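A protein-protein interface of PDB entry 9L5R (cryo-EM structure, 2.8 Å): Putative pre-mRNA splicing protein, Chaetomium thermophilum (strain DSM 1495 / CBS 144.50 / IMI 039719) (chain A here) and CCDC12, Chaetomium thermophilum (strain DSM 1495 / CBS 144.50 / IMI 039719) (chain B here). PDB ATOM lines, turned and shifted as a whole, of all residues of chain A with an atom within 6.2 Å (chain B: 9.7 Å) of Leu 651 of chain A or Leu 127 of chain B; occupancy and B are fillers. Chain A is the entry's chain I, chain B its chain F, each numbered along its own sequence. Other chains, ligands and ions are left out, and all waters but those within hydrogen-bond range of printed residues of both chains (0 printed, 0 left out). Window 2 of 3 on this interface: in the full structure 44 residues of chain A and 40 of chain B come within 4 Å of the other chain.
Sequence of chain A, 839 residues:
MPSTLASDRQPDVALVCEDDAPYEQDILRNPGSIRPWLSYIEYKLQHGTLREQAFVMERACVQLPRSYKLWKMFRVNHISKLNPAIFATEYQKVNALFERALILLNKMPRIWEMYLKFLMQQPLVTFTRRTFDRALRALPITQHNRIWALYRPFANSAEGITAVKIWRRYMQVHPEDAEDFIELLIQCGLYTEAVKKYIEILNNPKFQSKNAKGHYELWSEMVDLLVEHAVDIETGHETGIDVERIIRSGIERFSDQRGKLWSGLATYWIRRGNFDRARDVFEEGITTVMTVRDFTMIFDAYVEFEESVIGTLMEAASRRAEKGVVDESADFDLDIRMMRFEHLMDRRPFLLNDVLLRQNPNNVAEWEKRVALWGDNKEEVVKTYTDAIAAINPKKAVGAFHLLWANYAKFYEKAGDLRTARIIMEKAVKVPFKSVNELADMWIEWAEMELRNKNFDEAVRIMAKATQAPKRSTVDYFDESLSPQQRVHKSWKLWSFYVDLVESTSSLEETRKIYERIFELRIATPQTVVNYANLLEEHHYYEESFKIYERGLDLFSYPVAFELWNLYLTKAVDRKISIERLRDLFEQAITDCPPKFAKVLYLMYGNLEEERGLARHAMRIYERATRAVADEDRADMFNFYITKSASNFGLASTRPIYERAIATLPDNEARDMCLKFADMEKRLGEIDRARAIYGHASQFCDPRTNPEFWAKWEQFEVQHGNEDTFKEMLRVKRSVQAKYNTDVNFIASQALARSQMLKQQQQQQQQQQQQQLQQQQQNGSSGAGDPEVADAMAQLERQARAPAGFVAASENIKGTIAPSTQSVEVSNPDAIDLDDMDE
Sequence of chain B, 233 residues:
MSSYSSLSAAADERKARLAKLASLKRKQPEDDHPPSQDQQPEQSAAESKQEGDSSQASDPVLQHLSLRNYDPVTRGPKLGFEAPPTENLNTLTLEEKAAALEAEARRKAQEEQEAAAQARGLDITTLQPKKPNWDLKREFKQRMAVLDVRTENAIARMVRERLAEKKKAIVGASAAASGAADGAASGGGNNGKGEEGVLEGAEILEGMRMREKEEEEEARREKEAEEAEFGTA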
ATOM      1  N   SER A 645     -11.433  -3.674   6.625  1.00  0.00           N
ATOM      2  CA  SER A 645     -12.877  -3.854   6.580  1.00  0.00           C
ATOM      3  C   SER A 645     -13.439  -4.207   7.946  1.00  0.00           C
ATOM      4  O   SER A 645     -14.564  -3.818   8.268  1.00  0.00           O
ATOM      5  CB  SER A 645     -13.240  -4.933   5.564  1.00  0.00           C
ATOM      6  OG  SER A 645     -14.638  -5.148   5.535  1.00  0.00           O
ATOM      7  N   ALA A 646     -12.679  -4.940   8.761  1.00  0.00           N
ATOM      8  CA  ALA A 646     -13.109  -5.217  10.123  1.00  0.00           C
ATOM      9  C   ALA A 646     -13.057  -3.968  10.984  1.00  0.00           C
ATOM     10  O   ALA A 646     -13.882  -3.809  11.889  1.00  0.00           O
ATOM     11  CB  ALA A 646     -12.248  -6.321  10.732  1.00  0.00           C
ATOM     12  N   PHE A 649     -16.016  -1.622   9.387  1.00  0.00           N
ATOM     13  CA  PHE A 649     -17.322  -2.245   9.231  1.00  0.00           C
ATOM     14  C   PHE A 649     -17.390  -3.466  10.139  1.00  0.00           C
ATOM     15  O   PHE A 649     -16.586  -3.627  11.061  1.00  0.00           O
ATOM     16  CB  PHE A 649     -17.590  -2.643   7.773  1.00  0.00           C
ATOM     17  CG  PHE A 649     -17.752  -1.481   6.834  1.00  0.00           C
ATOM     18  CD1 PHE A 649     -18.988  -0.886   6.657  1.00  0.00           C
ATOM     19  CD2 PHE A 649     -16.670  -0.990   6.123  1.00  0.00           C
ATOM     20  CE1 PHE A 649     -19.140   0.182   5.793  1.00  0.00           C
ATOM     21  CE2 PHE A 649     -16.816   0.077   5.262  1.00  0.00           C
ATOM     22  CZ  PHE A 649     -18.052   0.662   5.097  1.00  0.00           C
ATOM     23  N   GLY A 650     -18.357  -4.340   9.871  1.00  0.00           N
ATOM     24  CA  GLY A 650     -18.560  -5.492  10.720  1.00  0.00           C
ATOM     25  C   GLY A 650     -17.869  -6.750  10.221  1.00  0.00           C
ATOM     26  O   GLY A 650     -17.490  -6.887   9.056  1.00  0.00           O
ATOM     27  N   LEU A 651     -17.712  -7.700  11.146  1.00  0.00           N
ATOM     28  CA  LEU A 651     -17.163  -9.005  10.798  1.00  0.00           C
ATOM     29  C   LEU A 651     -18.103  -9.779   9.881  1.00  0.00           C
ATOM     30  O   LEU A 651     -17.641 -10.545   9.019  1.00  0.00           O
ATOM     31  CB  LEU A 651     -16.873  -9.808  12.066  1.00  0.00           C
ATOM     32  CG  LEU A 651     -15.527  -9.612  12.778  1.00  0.00           C
ATOM     33  CD1 LEU A 651     -14.367  -9.946  11.859  1.00  0.00           C
ATOM     34  CD2 LEU A 651     -15.358  -8.219  13.367  1.00  0.00           C
ATOM     35  N   ALA A 652     -19.411  -9.565  10.031  1.00  0.00           N
ATOM     36  CA  ALA A 652     -20.369 -10.085   9.066  1.00  0.00           C
ATOM     37  C   ALA A 652     -20.137  -9.503   7.680  1.00  0.00           C
ATOM     38  O   ALA A 652     -20.452 -10.152   6.677  1.00  0.00           O
ATOM     39  CB  ALA A 652     -21.792  -9.793   9.535  1.00  0.00           C
ATOM     40  N   SER A 653     -19.586  -8.291   7.602  1.00  0.00           N
ATOM     41  CA  SER A 653     -19.196  -7.726   6.320  1.00  0.00           C
ATOM     42  C   SER A 653     -17.816  -8.183   5.871  1.00  0.00           C
ATOM     43  O   SER A 653     -17.492  -8.039   4.689  1.00  0.00           O
ATOM     44  CB  SER A 653     -19.216  -6.203   6.382  1.00  0.00           C
ATOM     45  OG  SER A 653     -18.032  -5.736   6.995  1.00  0.00           O
ATOM     46  N   THR A 654     -16.990  -8.705   6.773  1.00  0.00           N
ATOM     47  CA  THR A 654     -15.730  -9.299   6.345  1.00  0.00           C
ATOM     48  C   THR A 654     -15.879 -10.753   5.931  1.00  0.00           C
ATOM     49  O   THR A 654     -14.910 -11.344   5.449  1.00  0.00           O
ATOM     50  CB  THR A 654     -14.674  -9.216   7.443  1.00  0.00           C
ATOM     51  OG1 THR A 654     -15.065 -10.038   8.544  1.00  0.00           O
ATOM     52  CG2 THR A 654     -14.525  -7.793   7.913  1.00  0.00           C
ATOM     53  N   ARG A 655     -17.046 -11.349   6.165  1.00  0.00           N
ATOM     54  CA  ARG A 655     -17.304 -12.703   5.666  1.00  0.00           C
ATOM     55  C   ARG A 655     -17.132 -12.875   4.151  1.00  0.00           C
ATOM     56  O   ARG A 655     -16.432 -13.823   3.745  1.00  0.00           O
ATOM     57  CB  ARG A 655     -18.703 -13.158   6.100  1.00  0.00           C
ATOM     58  CG  ARG A 655     -18.858 -13.492   7.566  1.00  0.00           C
ATOM     59  CD  ARG A 655     -20.329 -13.585   7.911  1.00  0.00           C
ATOM     60  NE  ARG A 655     -20.567 -14.174   9.221  1.00  0.00           N
ATOM     61  CZ  ARG A 655     -21.742 -14.173   9.834  1.00  0.00           C
ATOM     62  NH1 ARG A 655     -22.805 -13.608   9.287  1.00  0.00           N
ATOM     63  NH2 ARG A 655     -21.854 -14.751  11.025  1.00  0.00           N
ATOM     64  N   PRO A 656     -17.728 -12.049   3.266  1.00  0.00           N
ATOM     65  CA  PRO A 656     -17.591 -12.344   1.827  1.00  0.00           C
ATOM     66  C   PRO A 656     -16.187 -12.140   1.299  1.00  0.00           C
ATOM     67  O   PRO A 656     -15.815 -12.774   0.302  1.00  0.00           O
ATOM     68  CB  PRO A 656     -18.584 -11.376   1.167  1.00  0.00           C
ATOM     69  CG  PRO A 656     -19.454 -10.899   2.260  1.00  0.00           C
ATOM     70  CD  PRO A 656     -18.564 -10.846   3.442  1.00  0.00           C
ATOM     71  N   TYR A 658     -13.539 -13.082   2.995  1.00  0.00           N
ATOM     72  CA  TYR A 658     -12.966 -14.385   3.310  1.00  0.00           C
ATOM     73  C   TYR A 658     -13.388 -15.431   2.291  1.00  0.00           C
ATOM     74  O   TYR A 658     -12.569 -16.250   1.855  1.00  0.00           O
ATOM     75  CB  TYR A 658     -13.398 -14.816   4.710  1.00  0.00           C
ATOM     76  CG  TYR A 658     -12.450 -14.425   5.811  1.00  0.00           C
ATOM     77  CD1 TYR A 658     -11.224 -15.046   5.944  1.00  0.00           C
ATOM     78  CD2 TYR A 658     -12.789 -13.440   6.724  1.00  0.00           C
ATOM     79  CE1 TYR A 658     -10.356 -14.695   6.952  1.00  0.00           C
ATOM     80  CE2 TYR A 658     -11.927 -13.082   7.736  1.00  0.00           C
ATOM     81  CZ  TYR A 658     -10.711 -13.713   7.845  1.00  0.00           C
ATOM     82  OH  TYR A 658      -9.844 -13.362   8.850  1.00  0.00           O
ATOM     83  N   MET A 680     -12.650 -16.939  12.946  1.00  0.00           N
ATOM     84  CA  MET A 680     -13.545 -15.792  13.048  1.00  0.00           C
ATOM     85  C   MET A 680     -14.990 -16.235  13.242  1.00  0.00           C
ATOM     86  O   MET A 680     -15.724 -15.651  14.048  1.00  0.00           O
ATOM     87  CB  MET A 680     -13.390 -14.914  11.803  1.00  0.00           C
ATOM     88  CG  MET A 680     -14.197 -13.620  11.778  1.00  0.00           C
ATOM     89  SD  MET A 680     -15.908 -13.727  11.221  1.00  0.00           S
ATOM     90  CE  MET A 680     -15.668 -13.993   9.472  1.00  0.00           C
ATOM     91  N   GLU A 681     -15.414 -17.278  12.525  1.00  0.00           N
ATOM     92  CA  GLU A 681     -16.787 -17.751  12.669  1.00  0.00           C
ATOM     93  C   GLU A 681     -17.017 -18.431  14.013  1.00  0.00           C
ATOM     94  O   GLU A 681     -18.115 -18.338  14.570  1.00  0.00           O
ATOM     95  CB  GLU A 681     -17.136 -18.693  11.521  1.00  0.00           C
ATOM     96  CG  GLU A 681     -17.402 -17.975  10.215  1.00  0.00           C
ATOM     97  CD  GLU A 681     -18.714 -17.228  10.225  1.00  0.00           C
ATOM     98  OE1 GLU A 681     -19.732 -17.825  10.626  1.00  0.00           O
ATOM     99  OE2 GLU A 681     -18.734 -16.045   9.832  1.00  0.00           O
ATOM    100  N   LEU A 684     -17.470 -15.604  16.400  1.00  0.00           N
ATOM    101  CA  LEU A 684     -18.844 -15.122  16.296  1.00  0.00           C
ATOM    102  C   LEU A 684     -19.842 -16.113  16.882  1.00  0.00           C
ATOM    103  O   LEU A 684     -20.942 -15.716  17.279  1.00  0.00           O
ATOM    104  CB  LEU A 684     -19.194 -14.808  14.844  1.00  0.00           C
ATOM    105  CG  LEU A 684     -19.020 -13.352  14.405  1.00  0.00           C
ATOM    106  CD1 LEU A 684     -17.561 -12.934  14.368  1.00  0.00           C
ATOM    107  CD2 LEU A 684     -19.668 -13.131  13.050  1.00  0.00           C
ATOM    108  N   GLU B 112      -4.701  -6.761  18.129  1.00  0.00           N
ATOM    109  CA  GLU B 112      -6.102  -7.139  18.267  1.00  0.00           C
ATOM    110  C   GLU B 112      -6.256  -8.626  18.554  1.00  0.00           C
ATOM    111  O   GLU B 112      -7.072  -9.017  19.402  1.00  0.00           O
ATOM    112  CB  GLU B 112      -6.873  -6.748  17.009  1.00  0.00           C
ATOM    113  CG  GLU B 112      -8.336  -7.118  17.059  1.00  0.00           C
ATOM    114  CD  GLU B 112      -9.067  -6.442  18.199  1.00  0.00           C
ATOM    115  OE1 GLU B 112      -8.809  -5.246  18.452  1.00  0.00           O
ATOM    116  OE2 GLU B 112      -9.892  -7.115  18.852  1.00  0.00           O
ATOM    117  N   GLY B 121     -13.700 -13.766  23.859  1.00  0.00           N
ATOM    118  CA  GLY B 121     -14.744 -13.817  22.858  1.00  0.00           C
ATOM    119  C   GLY B 121     -15.220 -12.456  22.401  1.00  0.00           C
ATOM    120  O   GLY B 121     -14.469 -11.477  22.445  1.00  0.00           O
ATOM    121  N   LEU B 122     -16.476 -12.383  21.970  1.00  0.00           N
ATOM    122  CA  LEU B 122     -16.995 -11.175  21.347  1.00  0.00           C
ATOM    123  C   LEU B 122     -17.242 -10.082  22.374  1.00  0.00           C
ATOM    124  O   LEU B 122     -17.886 -10.310  23.404  1.00  0.00           O
ATOM    125  CB  LEU B 122     -18.296 -11.470  20.605  1.00  0.00           C
ATOM    126  CG  LEU B 122     -18.204 -12.098  19.219  1.00  0.00           C
ATOM    127  CD1 LEU B 122     -19.597 -12.457  18.742  1.00  0.00           C
ATOM    128  CD2 LEU B 122     -17.520 -11.153  18.247  1.00  0.00           C
ATOM    129  N   ASP B 123     -16.724  -8.896  22.088  1.00  0.00           N
ATOM    130  CA  ASP B 123     -17.190  -7.662  22.691  1.00  0.00           C
ATOM    131  C   ASP B 123     -17.757  -6.759  21.602  1.00  0.00           C
ATOM    132  O   ASP B 123     -17.474  -6.935  20.414  1.00  0.00           O
ATOM    133  CB  ASP B 123     -16.079  -6.974  23.512  1.00  0.00           C
ATOM    134  CG  ASP B 123     -14.871  -6.562  22.680  1.00  0.00           C
ATOM    135  OD1 ASP B 123     -14.820  -6.826  21.465  1.00  0.00           O
ATOM    136  OD2 ASP B 123     -13.949  -5.955  23.264  1.00  0.00           O
ATOM    137  N   ILE B 124     -18.593  -5.810  22.022  1.00  0.00           N
ATOM    138  CA  ILE B 124     -19.316  -4.967  21.073  1.00  0.00           C
ATOM    139  C   ILE B 124     -18.355  -4.065  20.308  1.00  0.00           C
ATOM    140  O   ILE B 124     -18.497  -3.860  19.093  1.00  0.00           O
ATOM    141  CB  ILE B 124     -20.396  -4.163  21.818  1.00  0.00           C
ATOM    142  CG1 ILE B 124     -21.341  -5.117  22.551  1.00  0.00           C
ATOM    143  CG2 ILE B 124     -21.161  -3.268  20.871  1.00  0.00           C
ATOM    144  CD1 ILE B 124     -22.072  -6.076  21.633  1.00  0.00           C
ATOM    145  N   THR B 125     -17.330  -3.559  20.993  1.00  0.00           N
ATOM    146  CA  THR B 125     -16.384  -2.595  20.432  1.00  0.00           C
ATOM    147  C   THR B 125     -15.416  -3.221  19.437  1.00  0.00           C
ATOM    148  O   THR B 125     -14.576  -2.520  18.871  1.00  0.00           O
ATOM    149  CB  THR B 125     -15.624  -1.909  21.562  1.00  0.00           C
ATOM    150  OG1 THR B 125     -15.057  -2.898  22.428  1.00  0.00           O
ATOM    151  CG2 THR B 125     -16.560  -1.015  22.362  1.00  0.00           C
ATOM    152  N   THR B 126     -15.472  -4.537  19.231  1.00  0.00           N
ATOM    153  CA  THR B 126     -14.826  -5.149  18.072  1.00  0.00           C
ATOM    154  C   THR B 126     -15.784  -5.907  17.175  1.00  0.00           C
ATOM    155  O   THR B 126     -15.417  -6.197  16.032  1.00  0.00           O
ATOM    156  CB  THR B 126     -13.699  -6.100  18.494  1.00  0.00           C
ATOM    157  OG1 THR B 126     -14.249  -7.188  19.244  1.00  0.00           O
ATOM    158  CG2 THR B 126     -12.665  -5.370  19.337  1.00  0.00           C
ATOM    159  N   LEU B 127     -16.986  -6.256  17.636  1.00  0.00           N
ATOM    160  CA  LEU B 127     -18.001  -6.763  16.723  1.00  0.00           C
ATOM    161  C   LEU B 127     -18.430  -5.679  15.745  1.00  0.00           C
ATOM    162  O   LEU B 127     -18.769  -5.971  14.592  1.00  0.00           O
ATOM    163  CB  LEU B 127     -19.200  -7.295  17.512  1.00  0.00           C
ATOM    164  CG  LEU B 127     -20.402  -7.845  16.742  1.00  0.00           C
ATOM    165  CD1 LEU B 127     -20.860  -9.152  17.356  1.00  0.00           C
ATOM    166  CD2 LEU B 127     -21.548  -6.845  16.732  1.00  0.00           C
ATOM    167  N   GLN B 128     -18.416  -4.424  16.185  1.00  0.00           N
ATOM    168  CA  GLN B 128     -18.712  -3.289  15.310  1.00  0.00           C
ATOM    169  C   GLN B 128     -17.980  -2.074  15.853  1.00  0.00           C
ATOM    170  O   GLN B 128     -18.557  -1.240  16.561  1.00  0.00           O
ATOM    171  CB  GLN B 128     -20.215  -3.039  15.222  1.00  0.00           C
ATOM    172  CG  GLN B 128     -20.682  -2.558  13.871  1.00  0.00           C
ATOM    173  CD  GLN B 128     -20.701  -1.055  13.776  1.00  0.00           C
ATOM    174  OE1 GLN B 128     -20.874  -0.360  14.777  1.00  0.00           O
ATOM    175  NE2 GLN B 128     -20.515  -0.537  12.567  1.00  0.00           N
ATOM    176  N   PRO B 129     -16.692  -1.933  15.527  1.00  0.00           N
ATOM    177  CA  PRO B 129     -15.856  -0.960  16.250  1.00  0.00           C
ATOM    178  C   PRO B 129     -16.137   0.493  15.918  1.00  0.00           C
ATOM    179  O   PRO B 129     -16.042   1.342  16.813  1.00  0.00           O
ATOM    180  CB  PRO B 129     -14.429  -1.373  15.854  1.00  0.00           C
ATOM    181  CG  PRO B 129     -14.594  -2.396  14.722  1.00  0.00           C
ATOM    182  CD  PRO B 129     -16.023  -2.364  14.293  1.00  0.00           C
ATOM    183  N   LYS B 130     -16.475   0.816  14.676  1.00  0.00           N
ATOM    184  CA  LYS B 130     -16.860   2.170  14.313  1.00  0.00           C
ATOM    185  C   LYS B 130     -18.302   2.141  13.843  1.00  0.00           C
ATOM    186  O   LYS B 130     -18.711   1.208  13.145  1.00  0.00           O
ATOM    187  CB  LYS B 130     -15.937   2.750  13.239  1.00  0.00           C
ATOM    188  CG  LYS B 130     -14.561   3.121  13.775  1.00  0.00           C
ATOM    189  CD  LYS B 130     -13.719   3.843  12.738  1.00  0.00           C
ATOM    190  CE  LYS B 130     -13.161   2.871  11.720  1.00  0.00           C
ATOM    191  NZ  LYS B 130     -12.210   3.523  10.782  1.00  0.00           N
ATOM    192  N   LYS B 131     -19.057   3.153  14.242  1.00  0.00           N
ATOM    193  CA  LYS B 131     -20.494   3.289  14.051  1.00  0.00           C
ATOM    194  C   LYS B 131     -20.819   3.261  12.563  1.00  0.00           C
ATOM    195  O   LYS B 131     -20.016   3.748  11.757  1.00  0.00           O
ATOM    196  CB  LYS B 131     -20.946   4.591  14.716  1.00  0.00           C
ATOM    197  CG  LYS B 131     -22.431   4.842  14.794  1.00  0.00           C
ATOM    198  CD  LYS B 131     -22.686   6.096  15.600  1.00  0.00           C
ATOM    199  CE  LYS B 131     -24.161   6.376  15.736  1.00  0.00           C
ATOM    200  NZ  LYS B 131     -24.388   7.599  16.541  1.00  0.00           N
ATOM    201  N   PRO B 132     -21.927   2.644  12.150  1.00  0.00           N
ATOM    202  CA  PRO B 132     -22.282   2.650  10.726  1.00  0.00           C
ATOM    203  C   PRO B 132     -22.517   4.058  10.210  1.00  0.00           C
ATOM    204  O   PRO B 132     -23.020   4.929  10.925  1.00  0.00           O
ATOM    205  CB  PRO B 132     -23.569   1.817  10.676  1.00  0.00           C
ATOM    206  CG  PRO B 132     -24.085   1.819  12.077  1.00  0.00           C
ATOM    207  CD  PRO B 132     -22.861   1.821  12.933  1.00  0.00           C
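The side-chain hydroxyl (OG1) of Thr 654 of chain A lies within hydrogen-bond range of the backbone carbonyl oxygen (O) of Leu 651 of chain A (2.7 Å). The side-chain carboxylate (OD1) of Asp 123 of chain B sits close to the backbone NH (N) of Thr 126 of chain B (3.3 Å). OG of Ser 653 of chain A sits at hydrogen-bond distance from O of Gly 650 of chain A (2.4 Å).
Of the printed residues of chain B, Leu 651 of chain A touches Thr 126 and Leu 127. Printed residues of chain A within 4 Å of Leu 127 of chain B: Gly 650 and Leu 651. Gly 650 of chain A touches one residue of chain B. No residue of chain B comes within 4 Å of Ala 652 of chain A. No residue of chain B comes within 4 Å of Ser 653 of chain A. No residue of chain B comes within 4 Å of Thr 654 of chain A. Of the printed residues of chain B, Ala 646 of chain A touches Pro 129. Of the printed residues of chain B, Leu 684 of chain A touches Leu 122 (3.7 Å). Of the printed residues of chain A, Pro 129 of chain B touches Ala 646 and Phe 649. Of the printed residues of chain A, Leu 122 of chain B touches Leu 684. Ser 645 of chain A touches none of the printed residues of chain B. The nearest printed residue of chain B that does not touch Leu 651 of chain A is Gln 128 of chain B (5.6 Å). The nearest printed residue of chain A that does not touch Leu 127 of chain B is Phe 649 of chain A (4.8 Å). The nearest printed residue of chain B that does not touch Ala 646 of chain A is Thr 126 of chain B (5.0 Å).
Pro 129 of chain B touches Ala 646 of chain A. Phe 649 of chain A touches Pro 129 of chain B (O to CD, 3.5 Å). Gly 650 of chain A touches Leu 127 of chain B (CA to O, 3.9 Å). Leu 651 of chain A touches Thr 126 of chain B (CD2 to O, 3.3 Å). Leu 651 of chain A touches Leu 127 of chain B. Leu 122 of chain B touches Leu 684 of chain A.
Hydrophobic or aromatic side chains of chain B within 4 Å of the printed part of chain A: Leu 122 and Pro 129. Of the 14 printed residues of chain A, 5 touch a printed residue of chain B. Hydrophobic or aromatic side chains of chain A within 4 Å of the printed part of chain B: Leu 651. Among the printed residues, no Asp or Glu carboxylate lies within 4 Å of a Lys or Arg side-chain nitrogen of the other chain.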
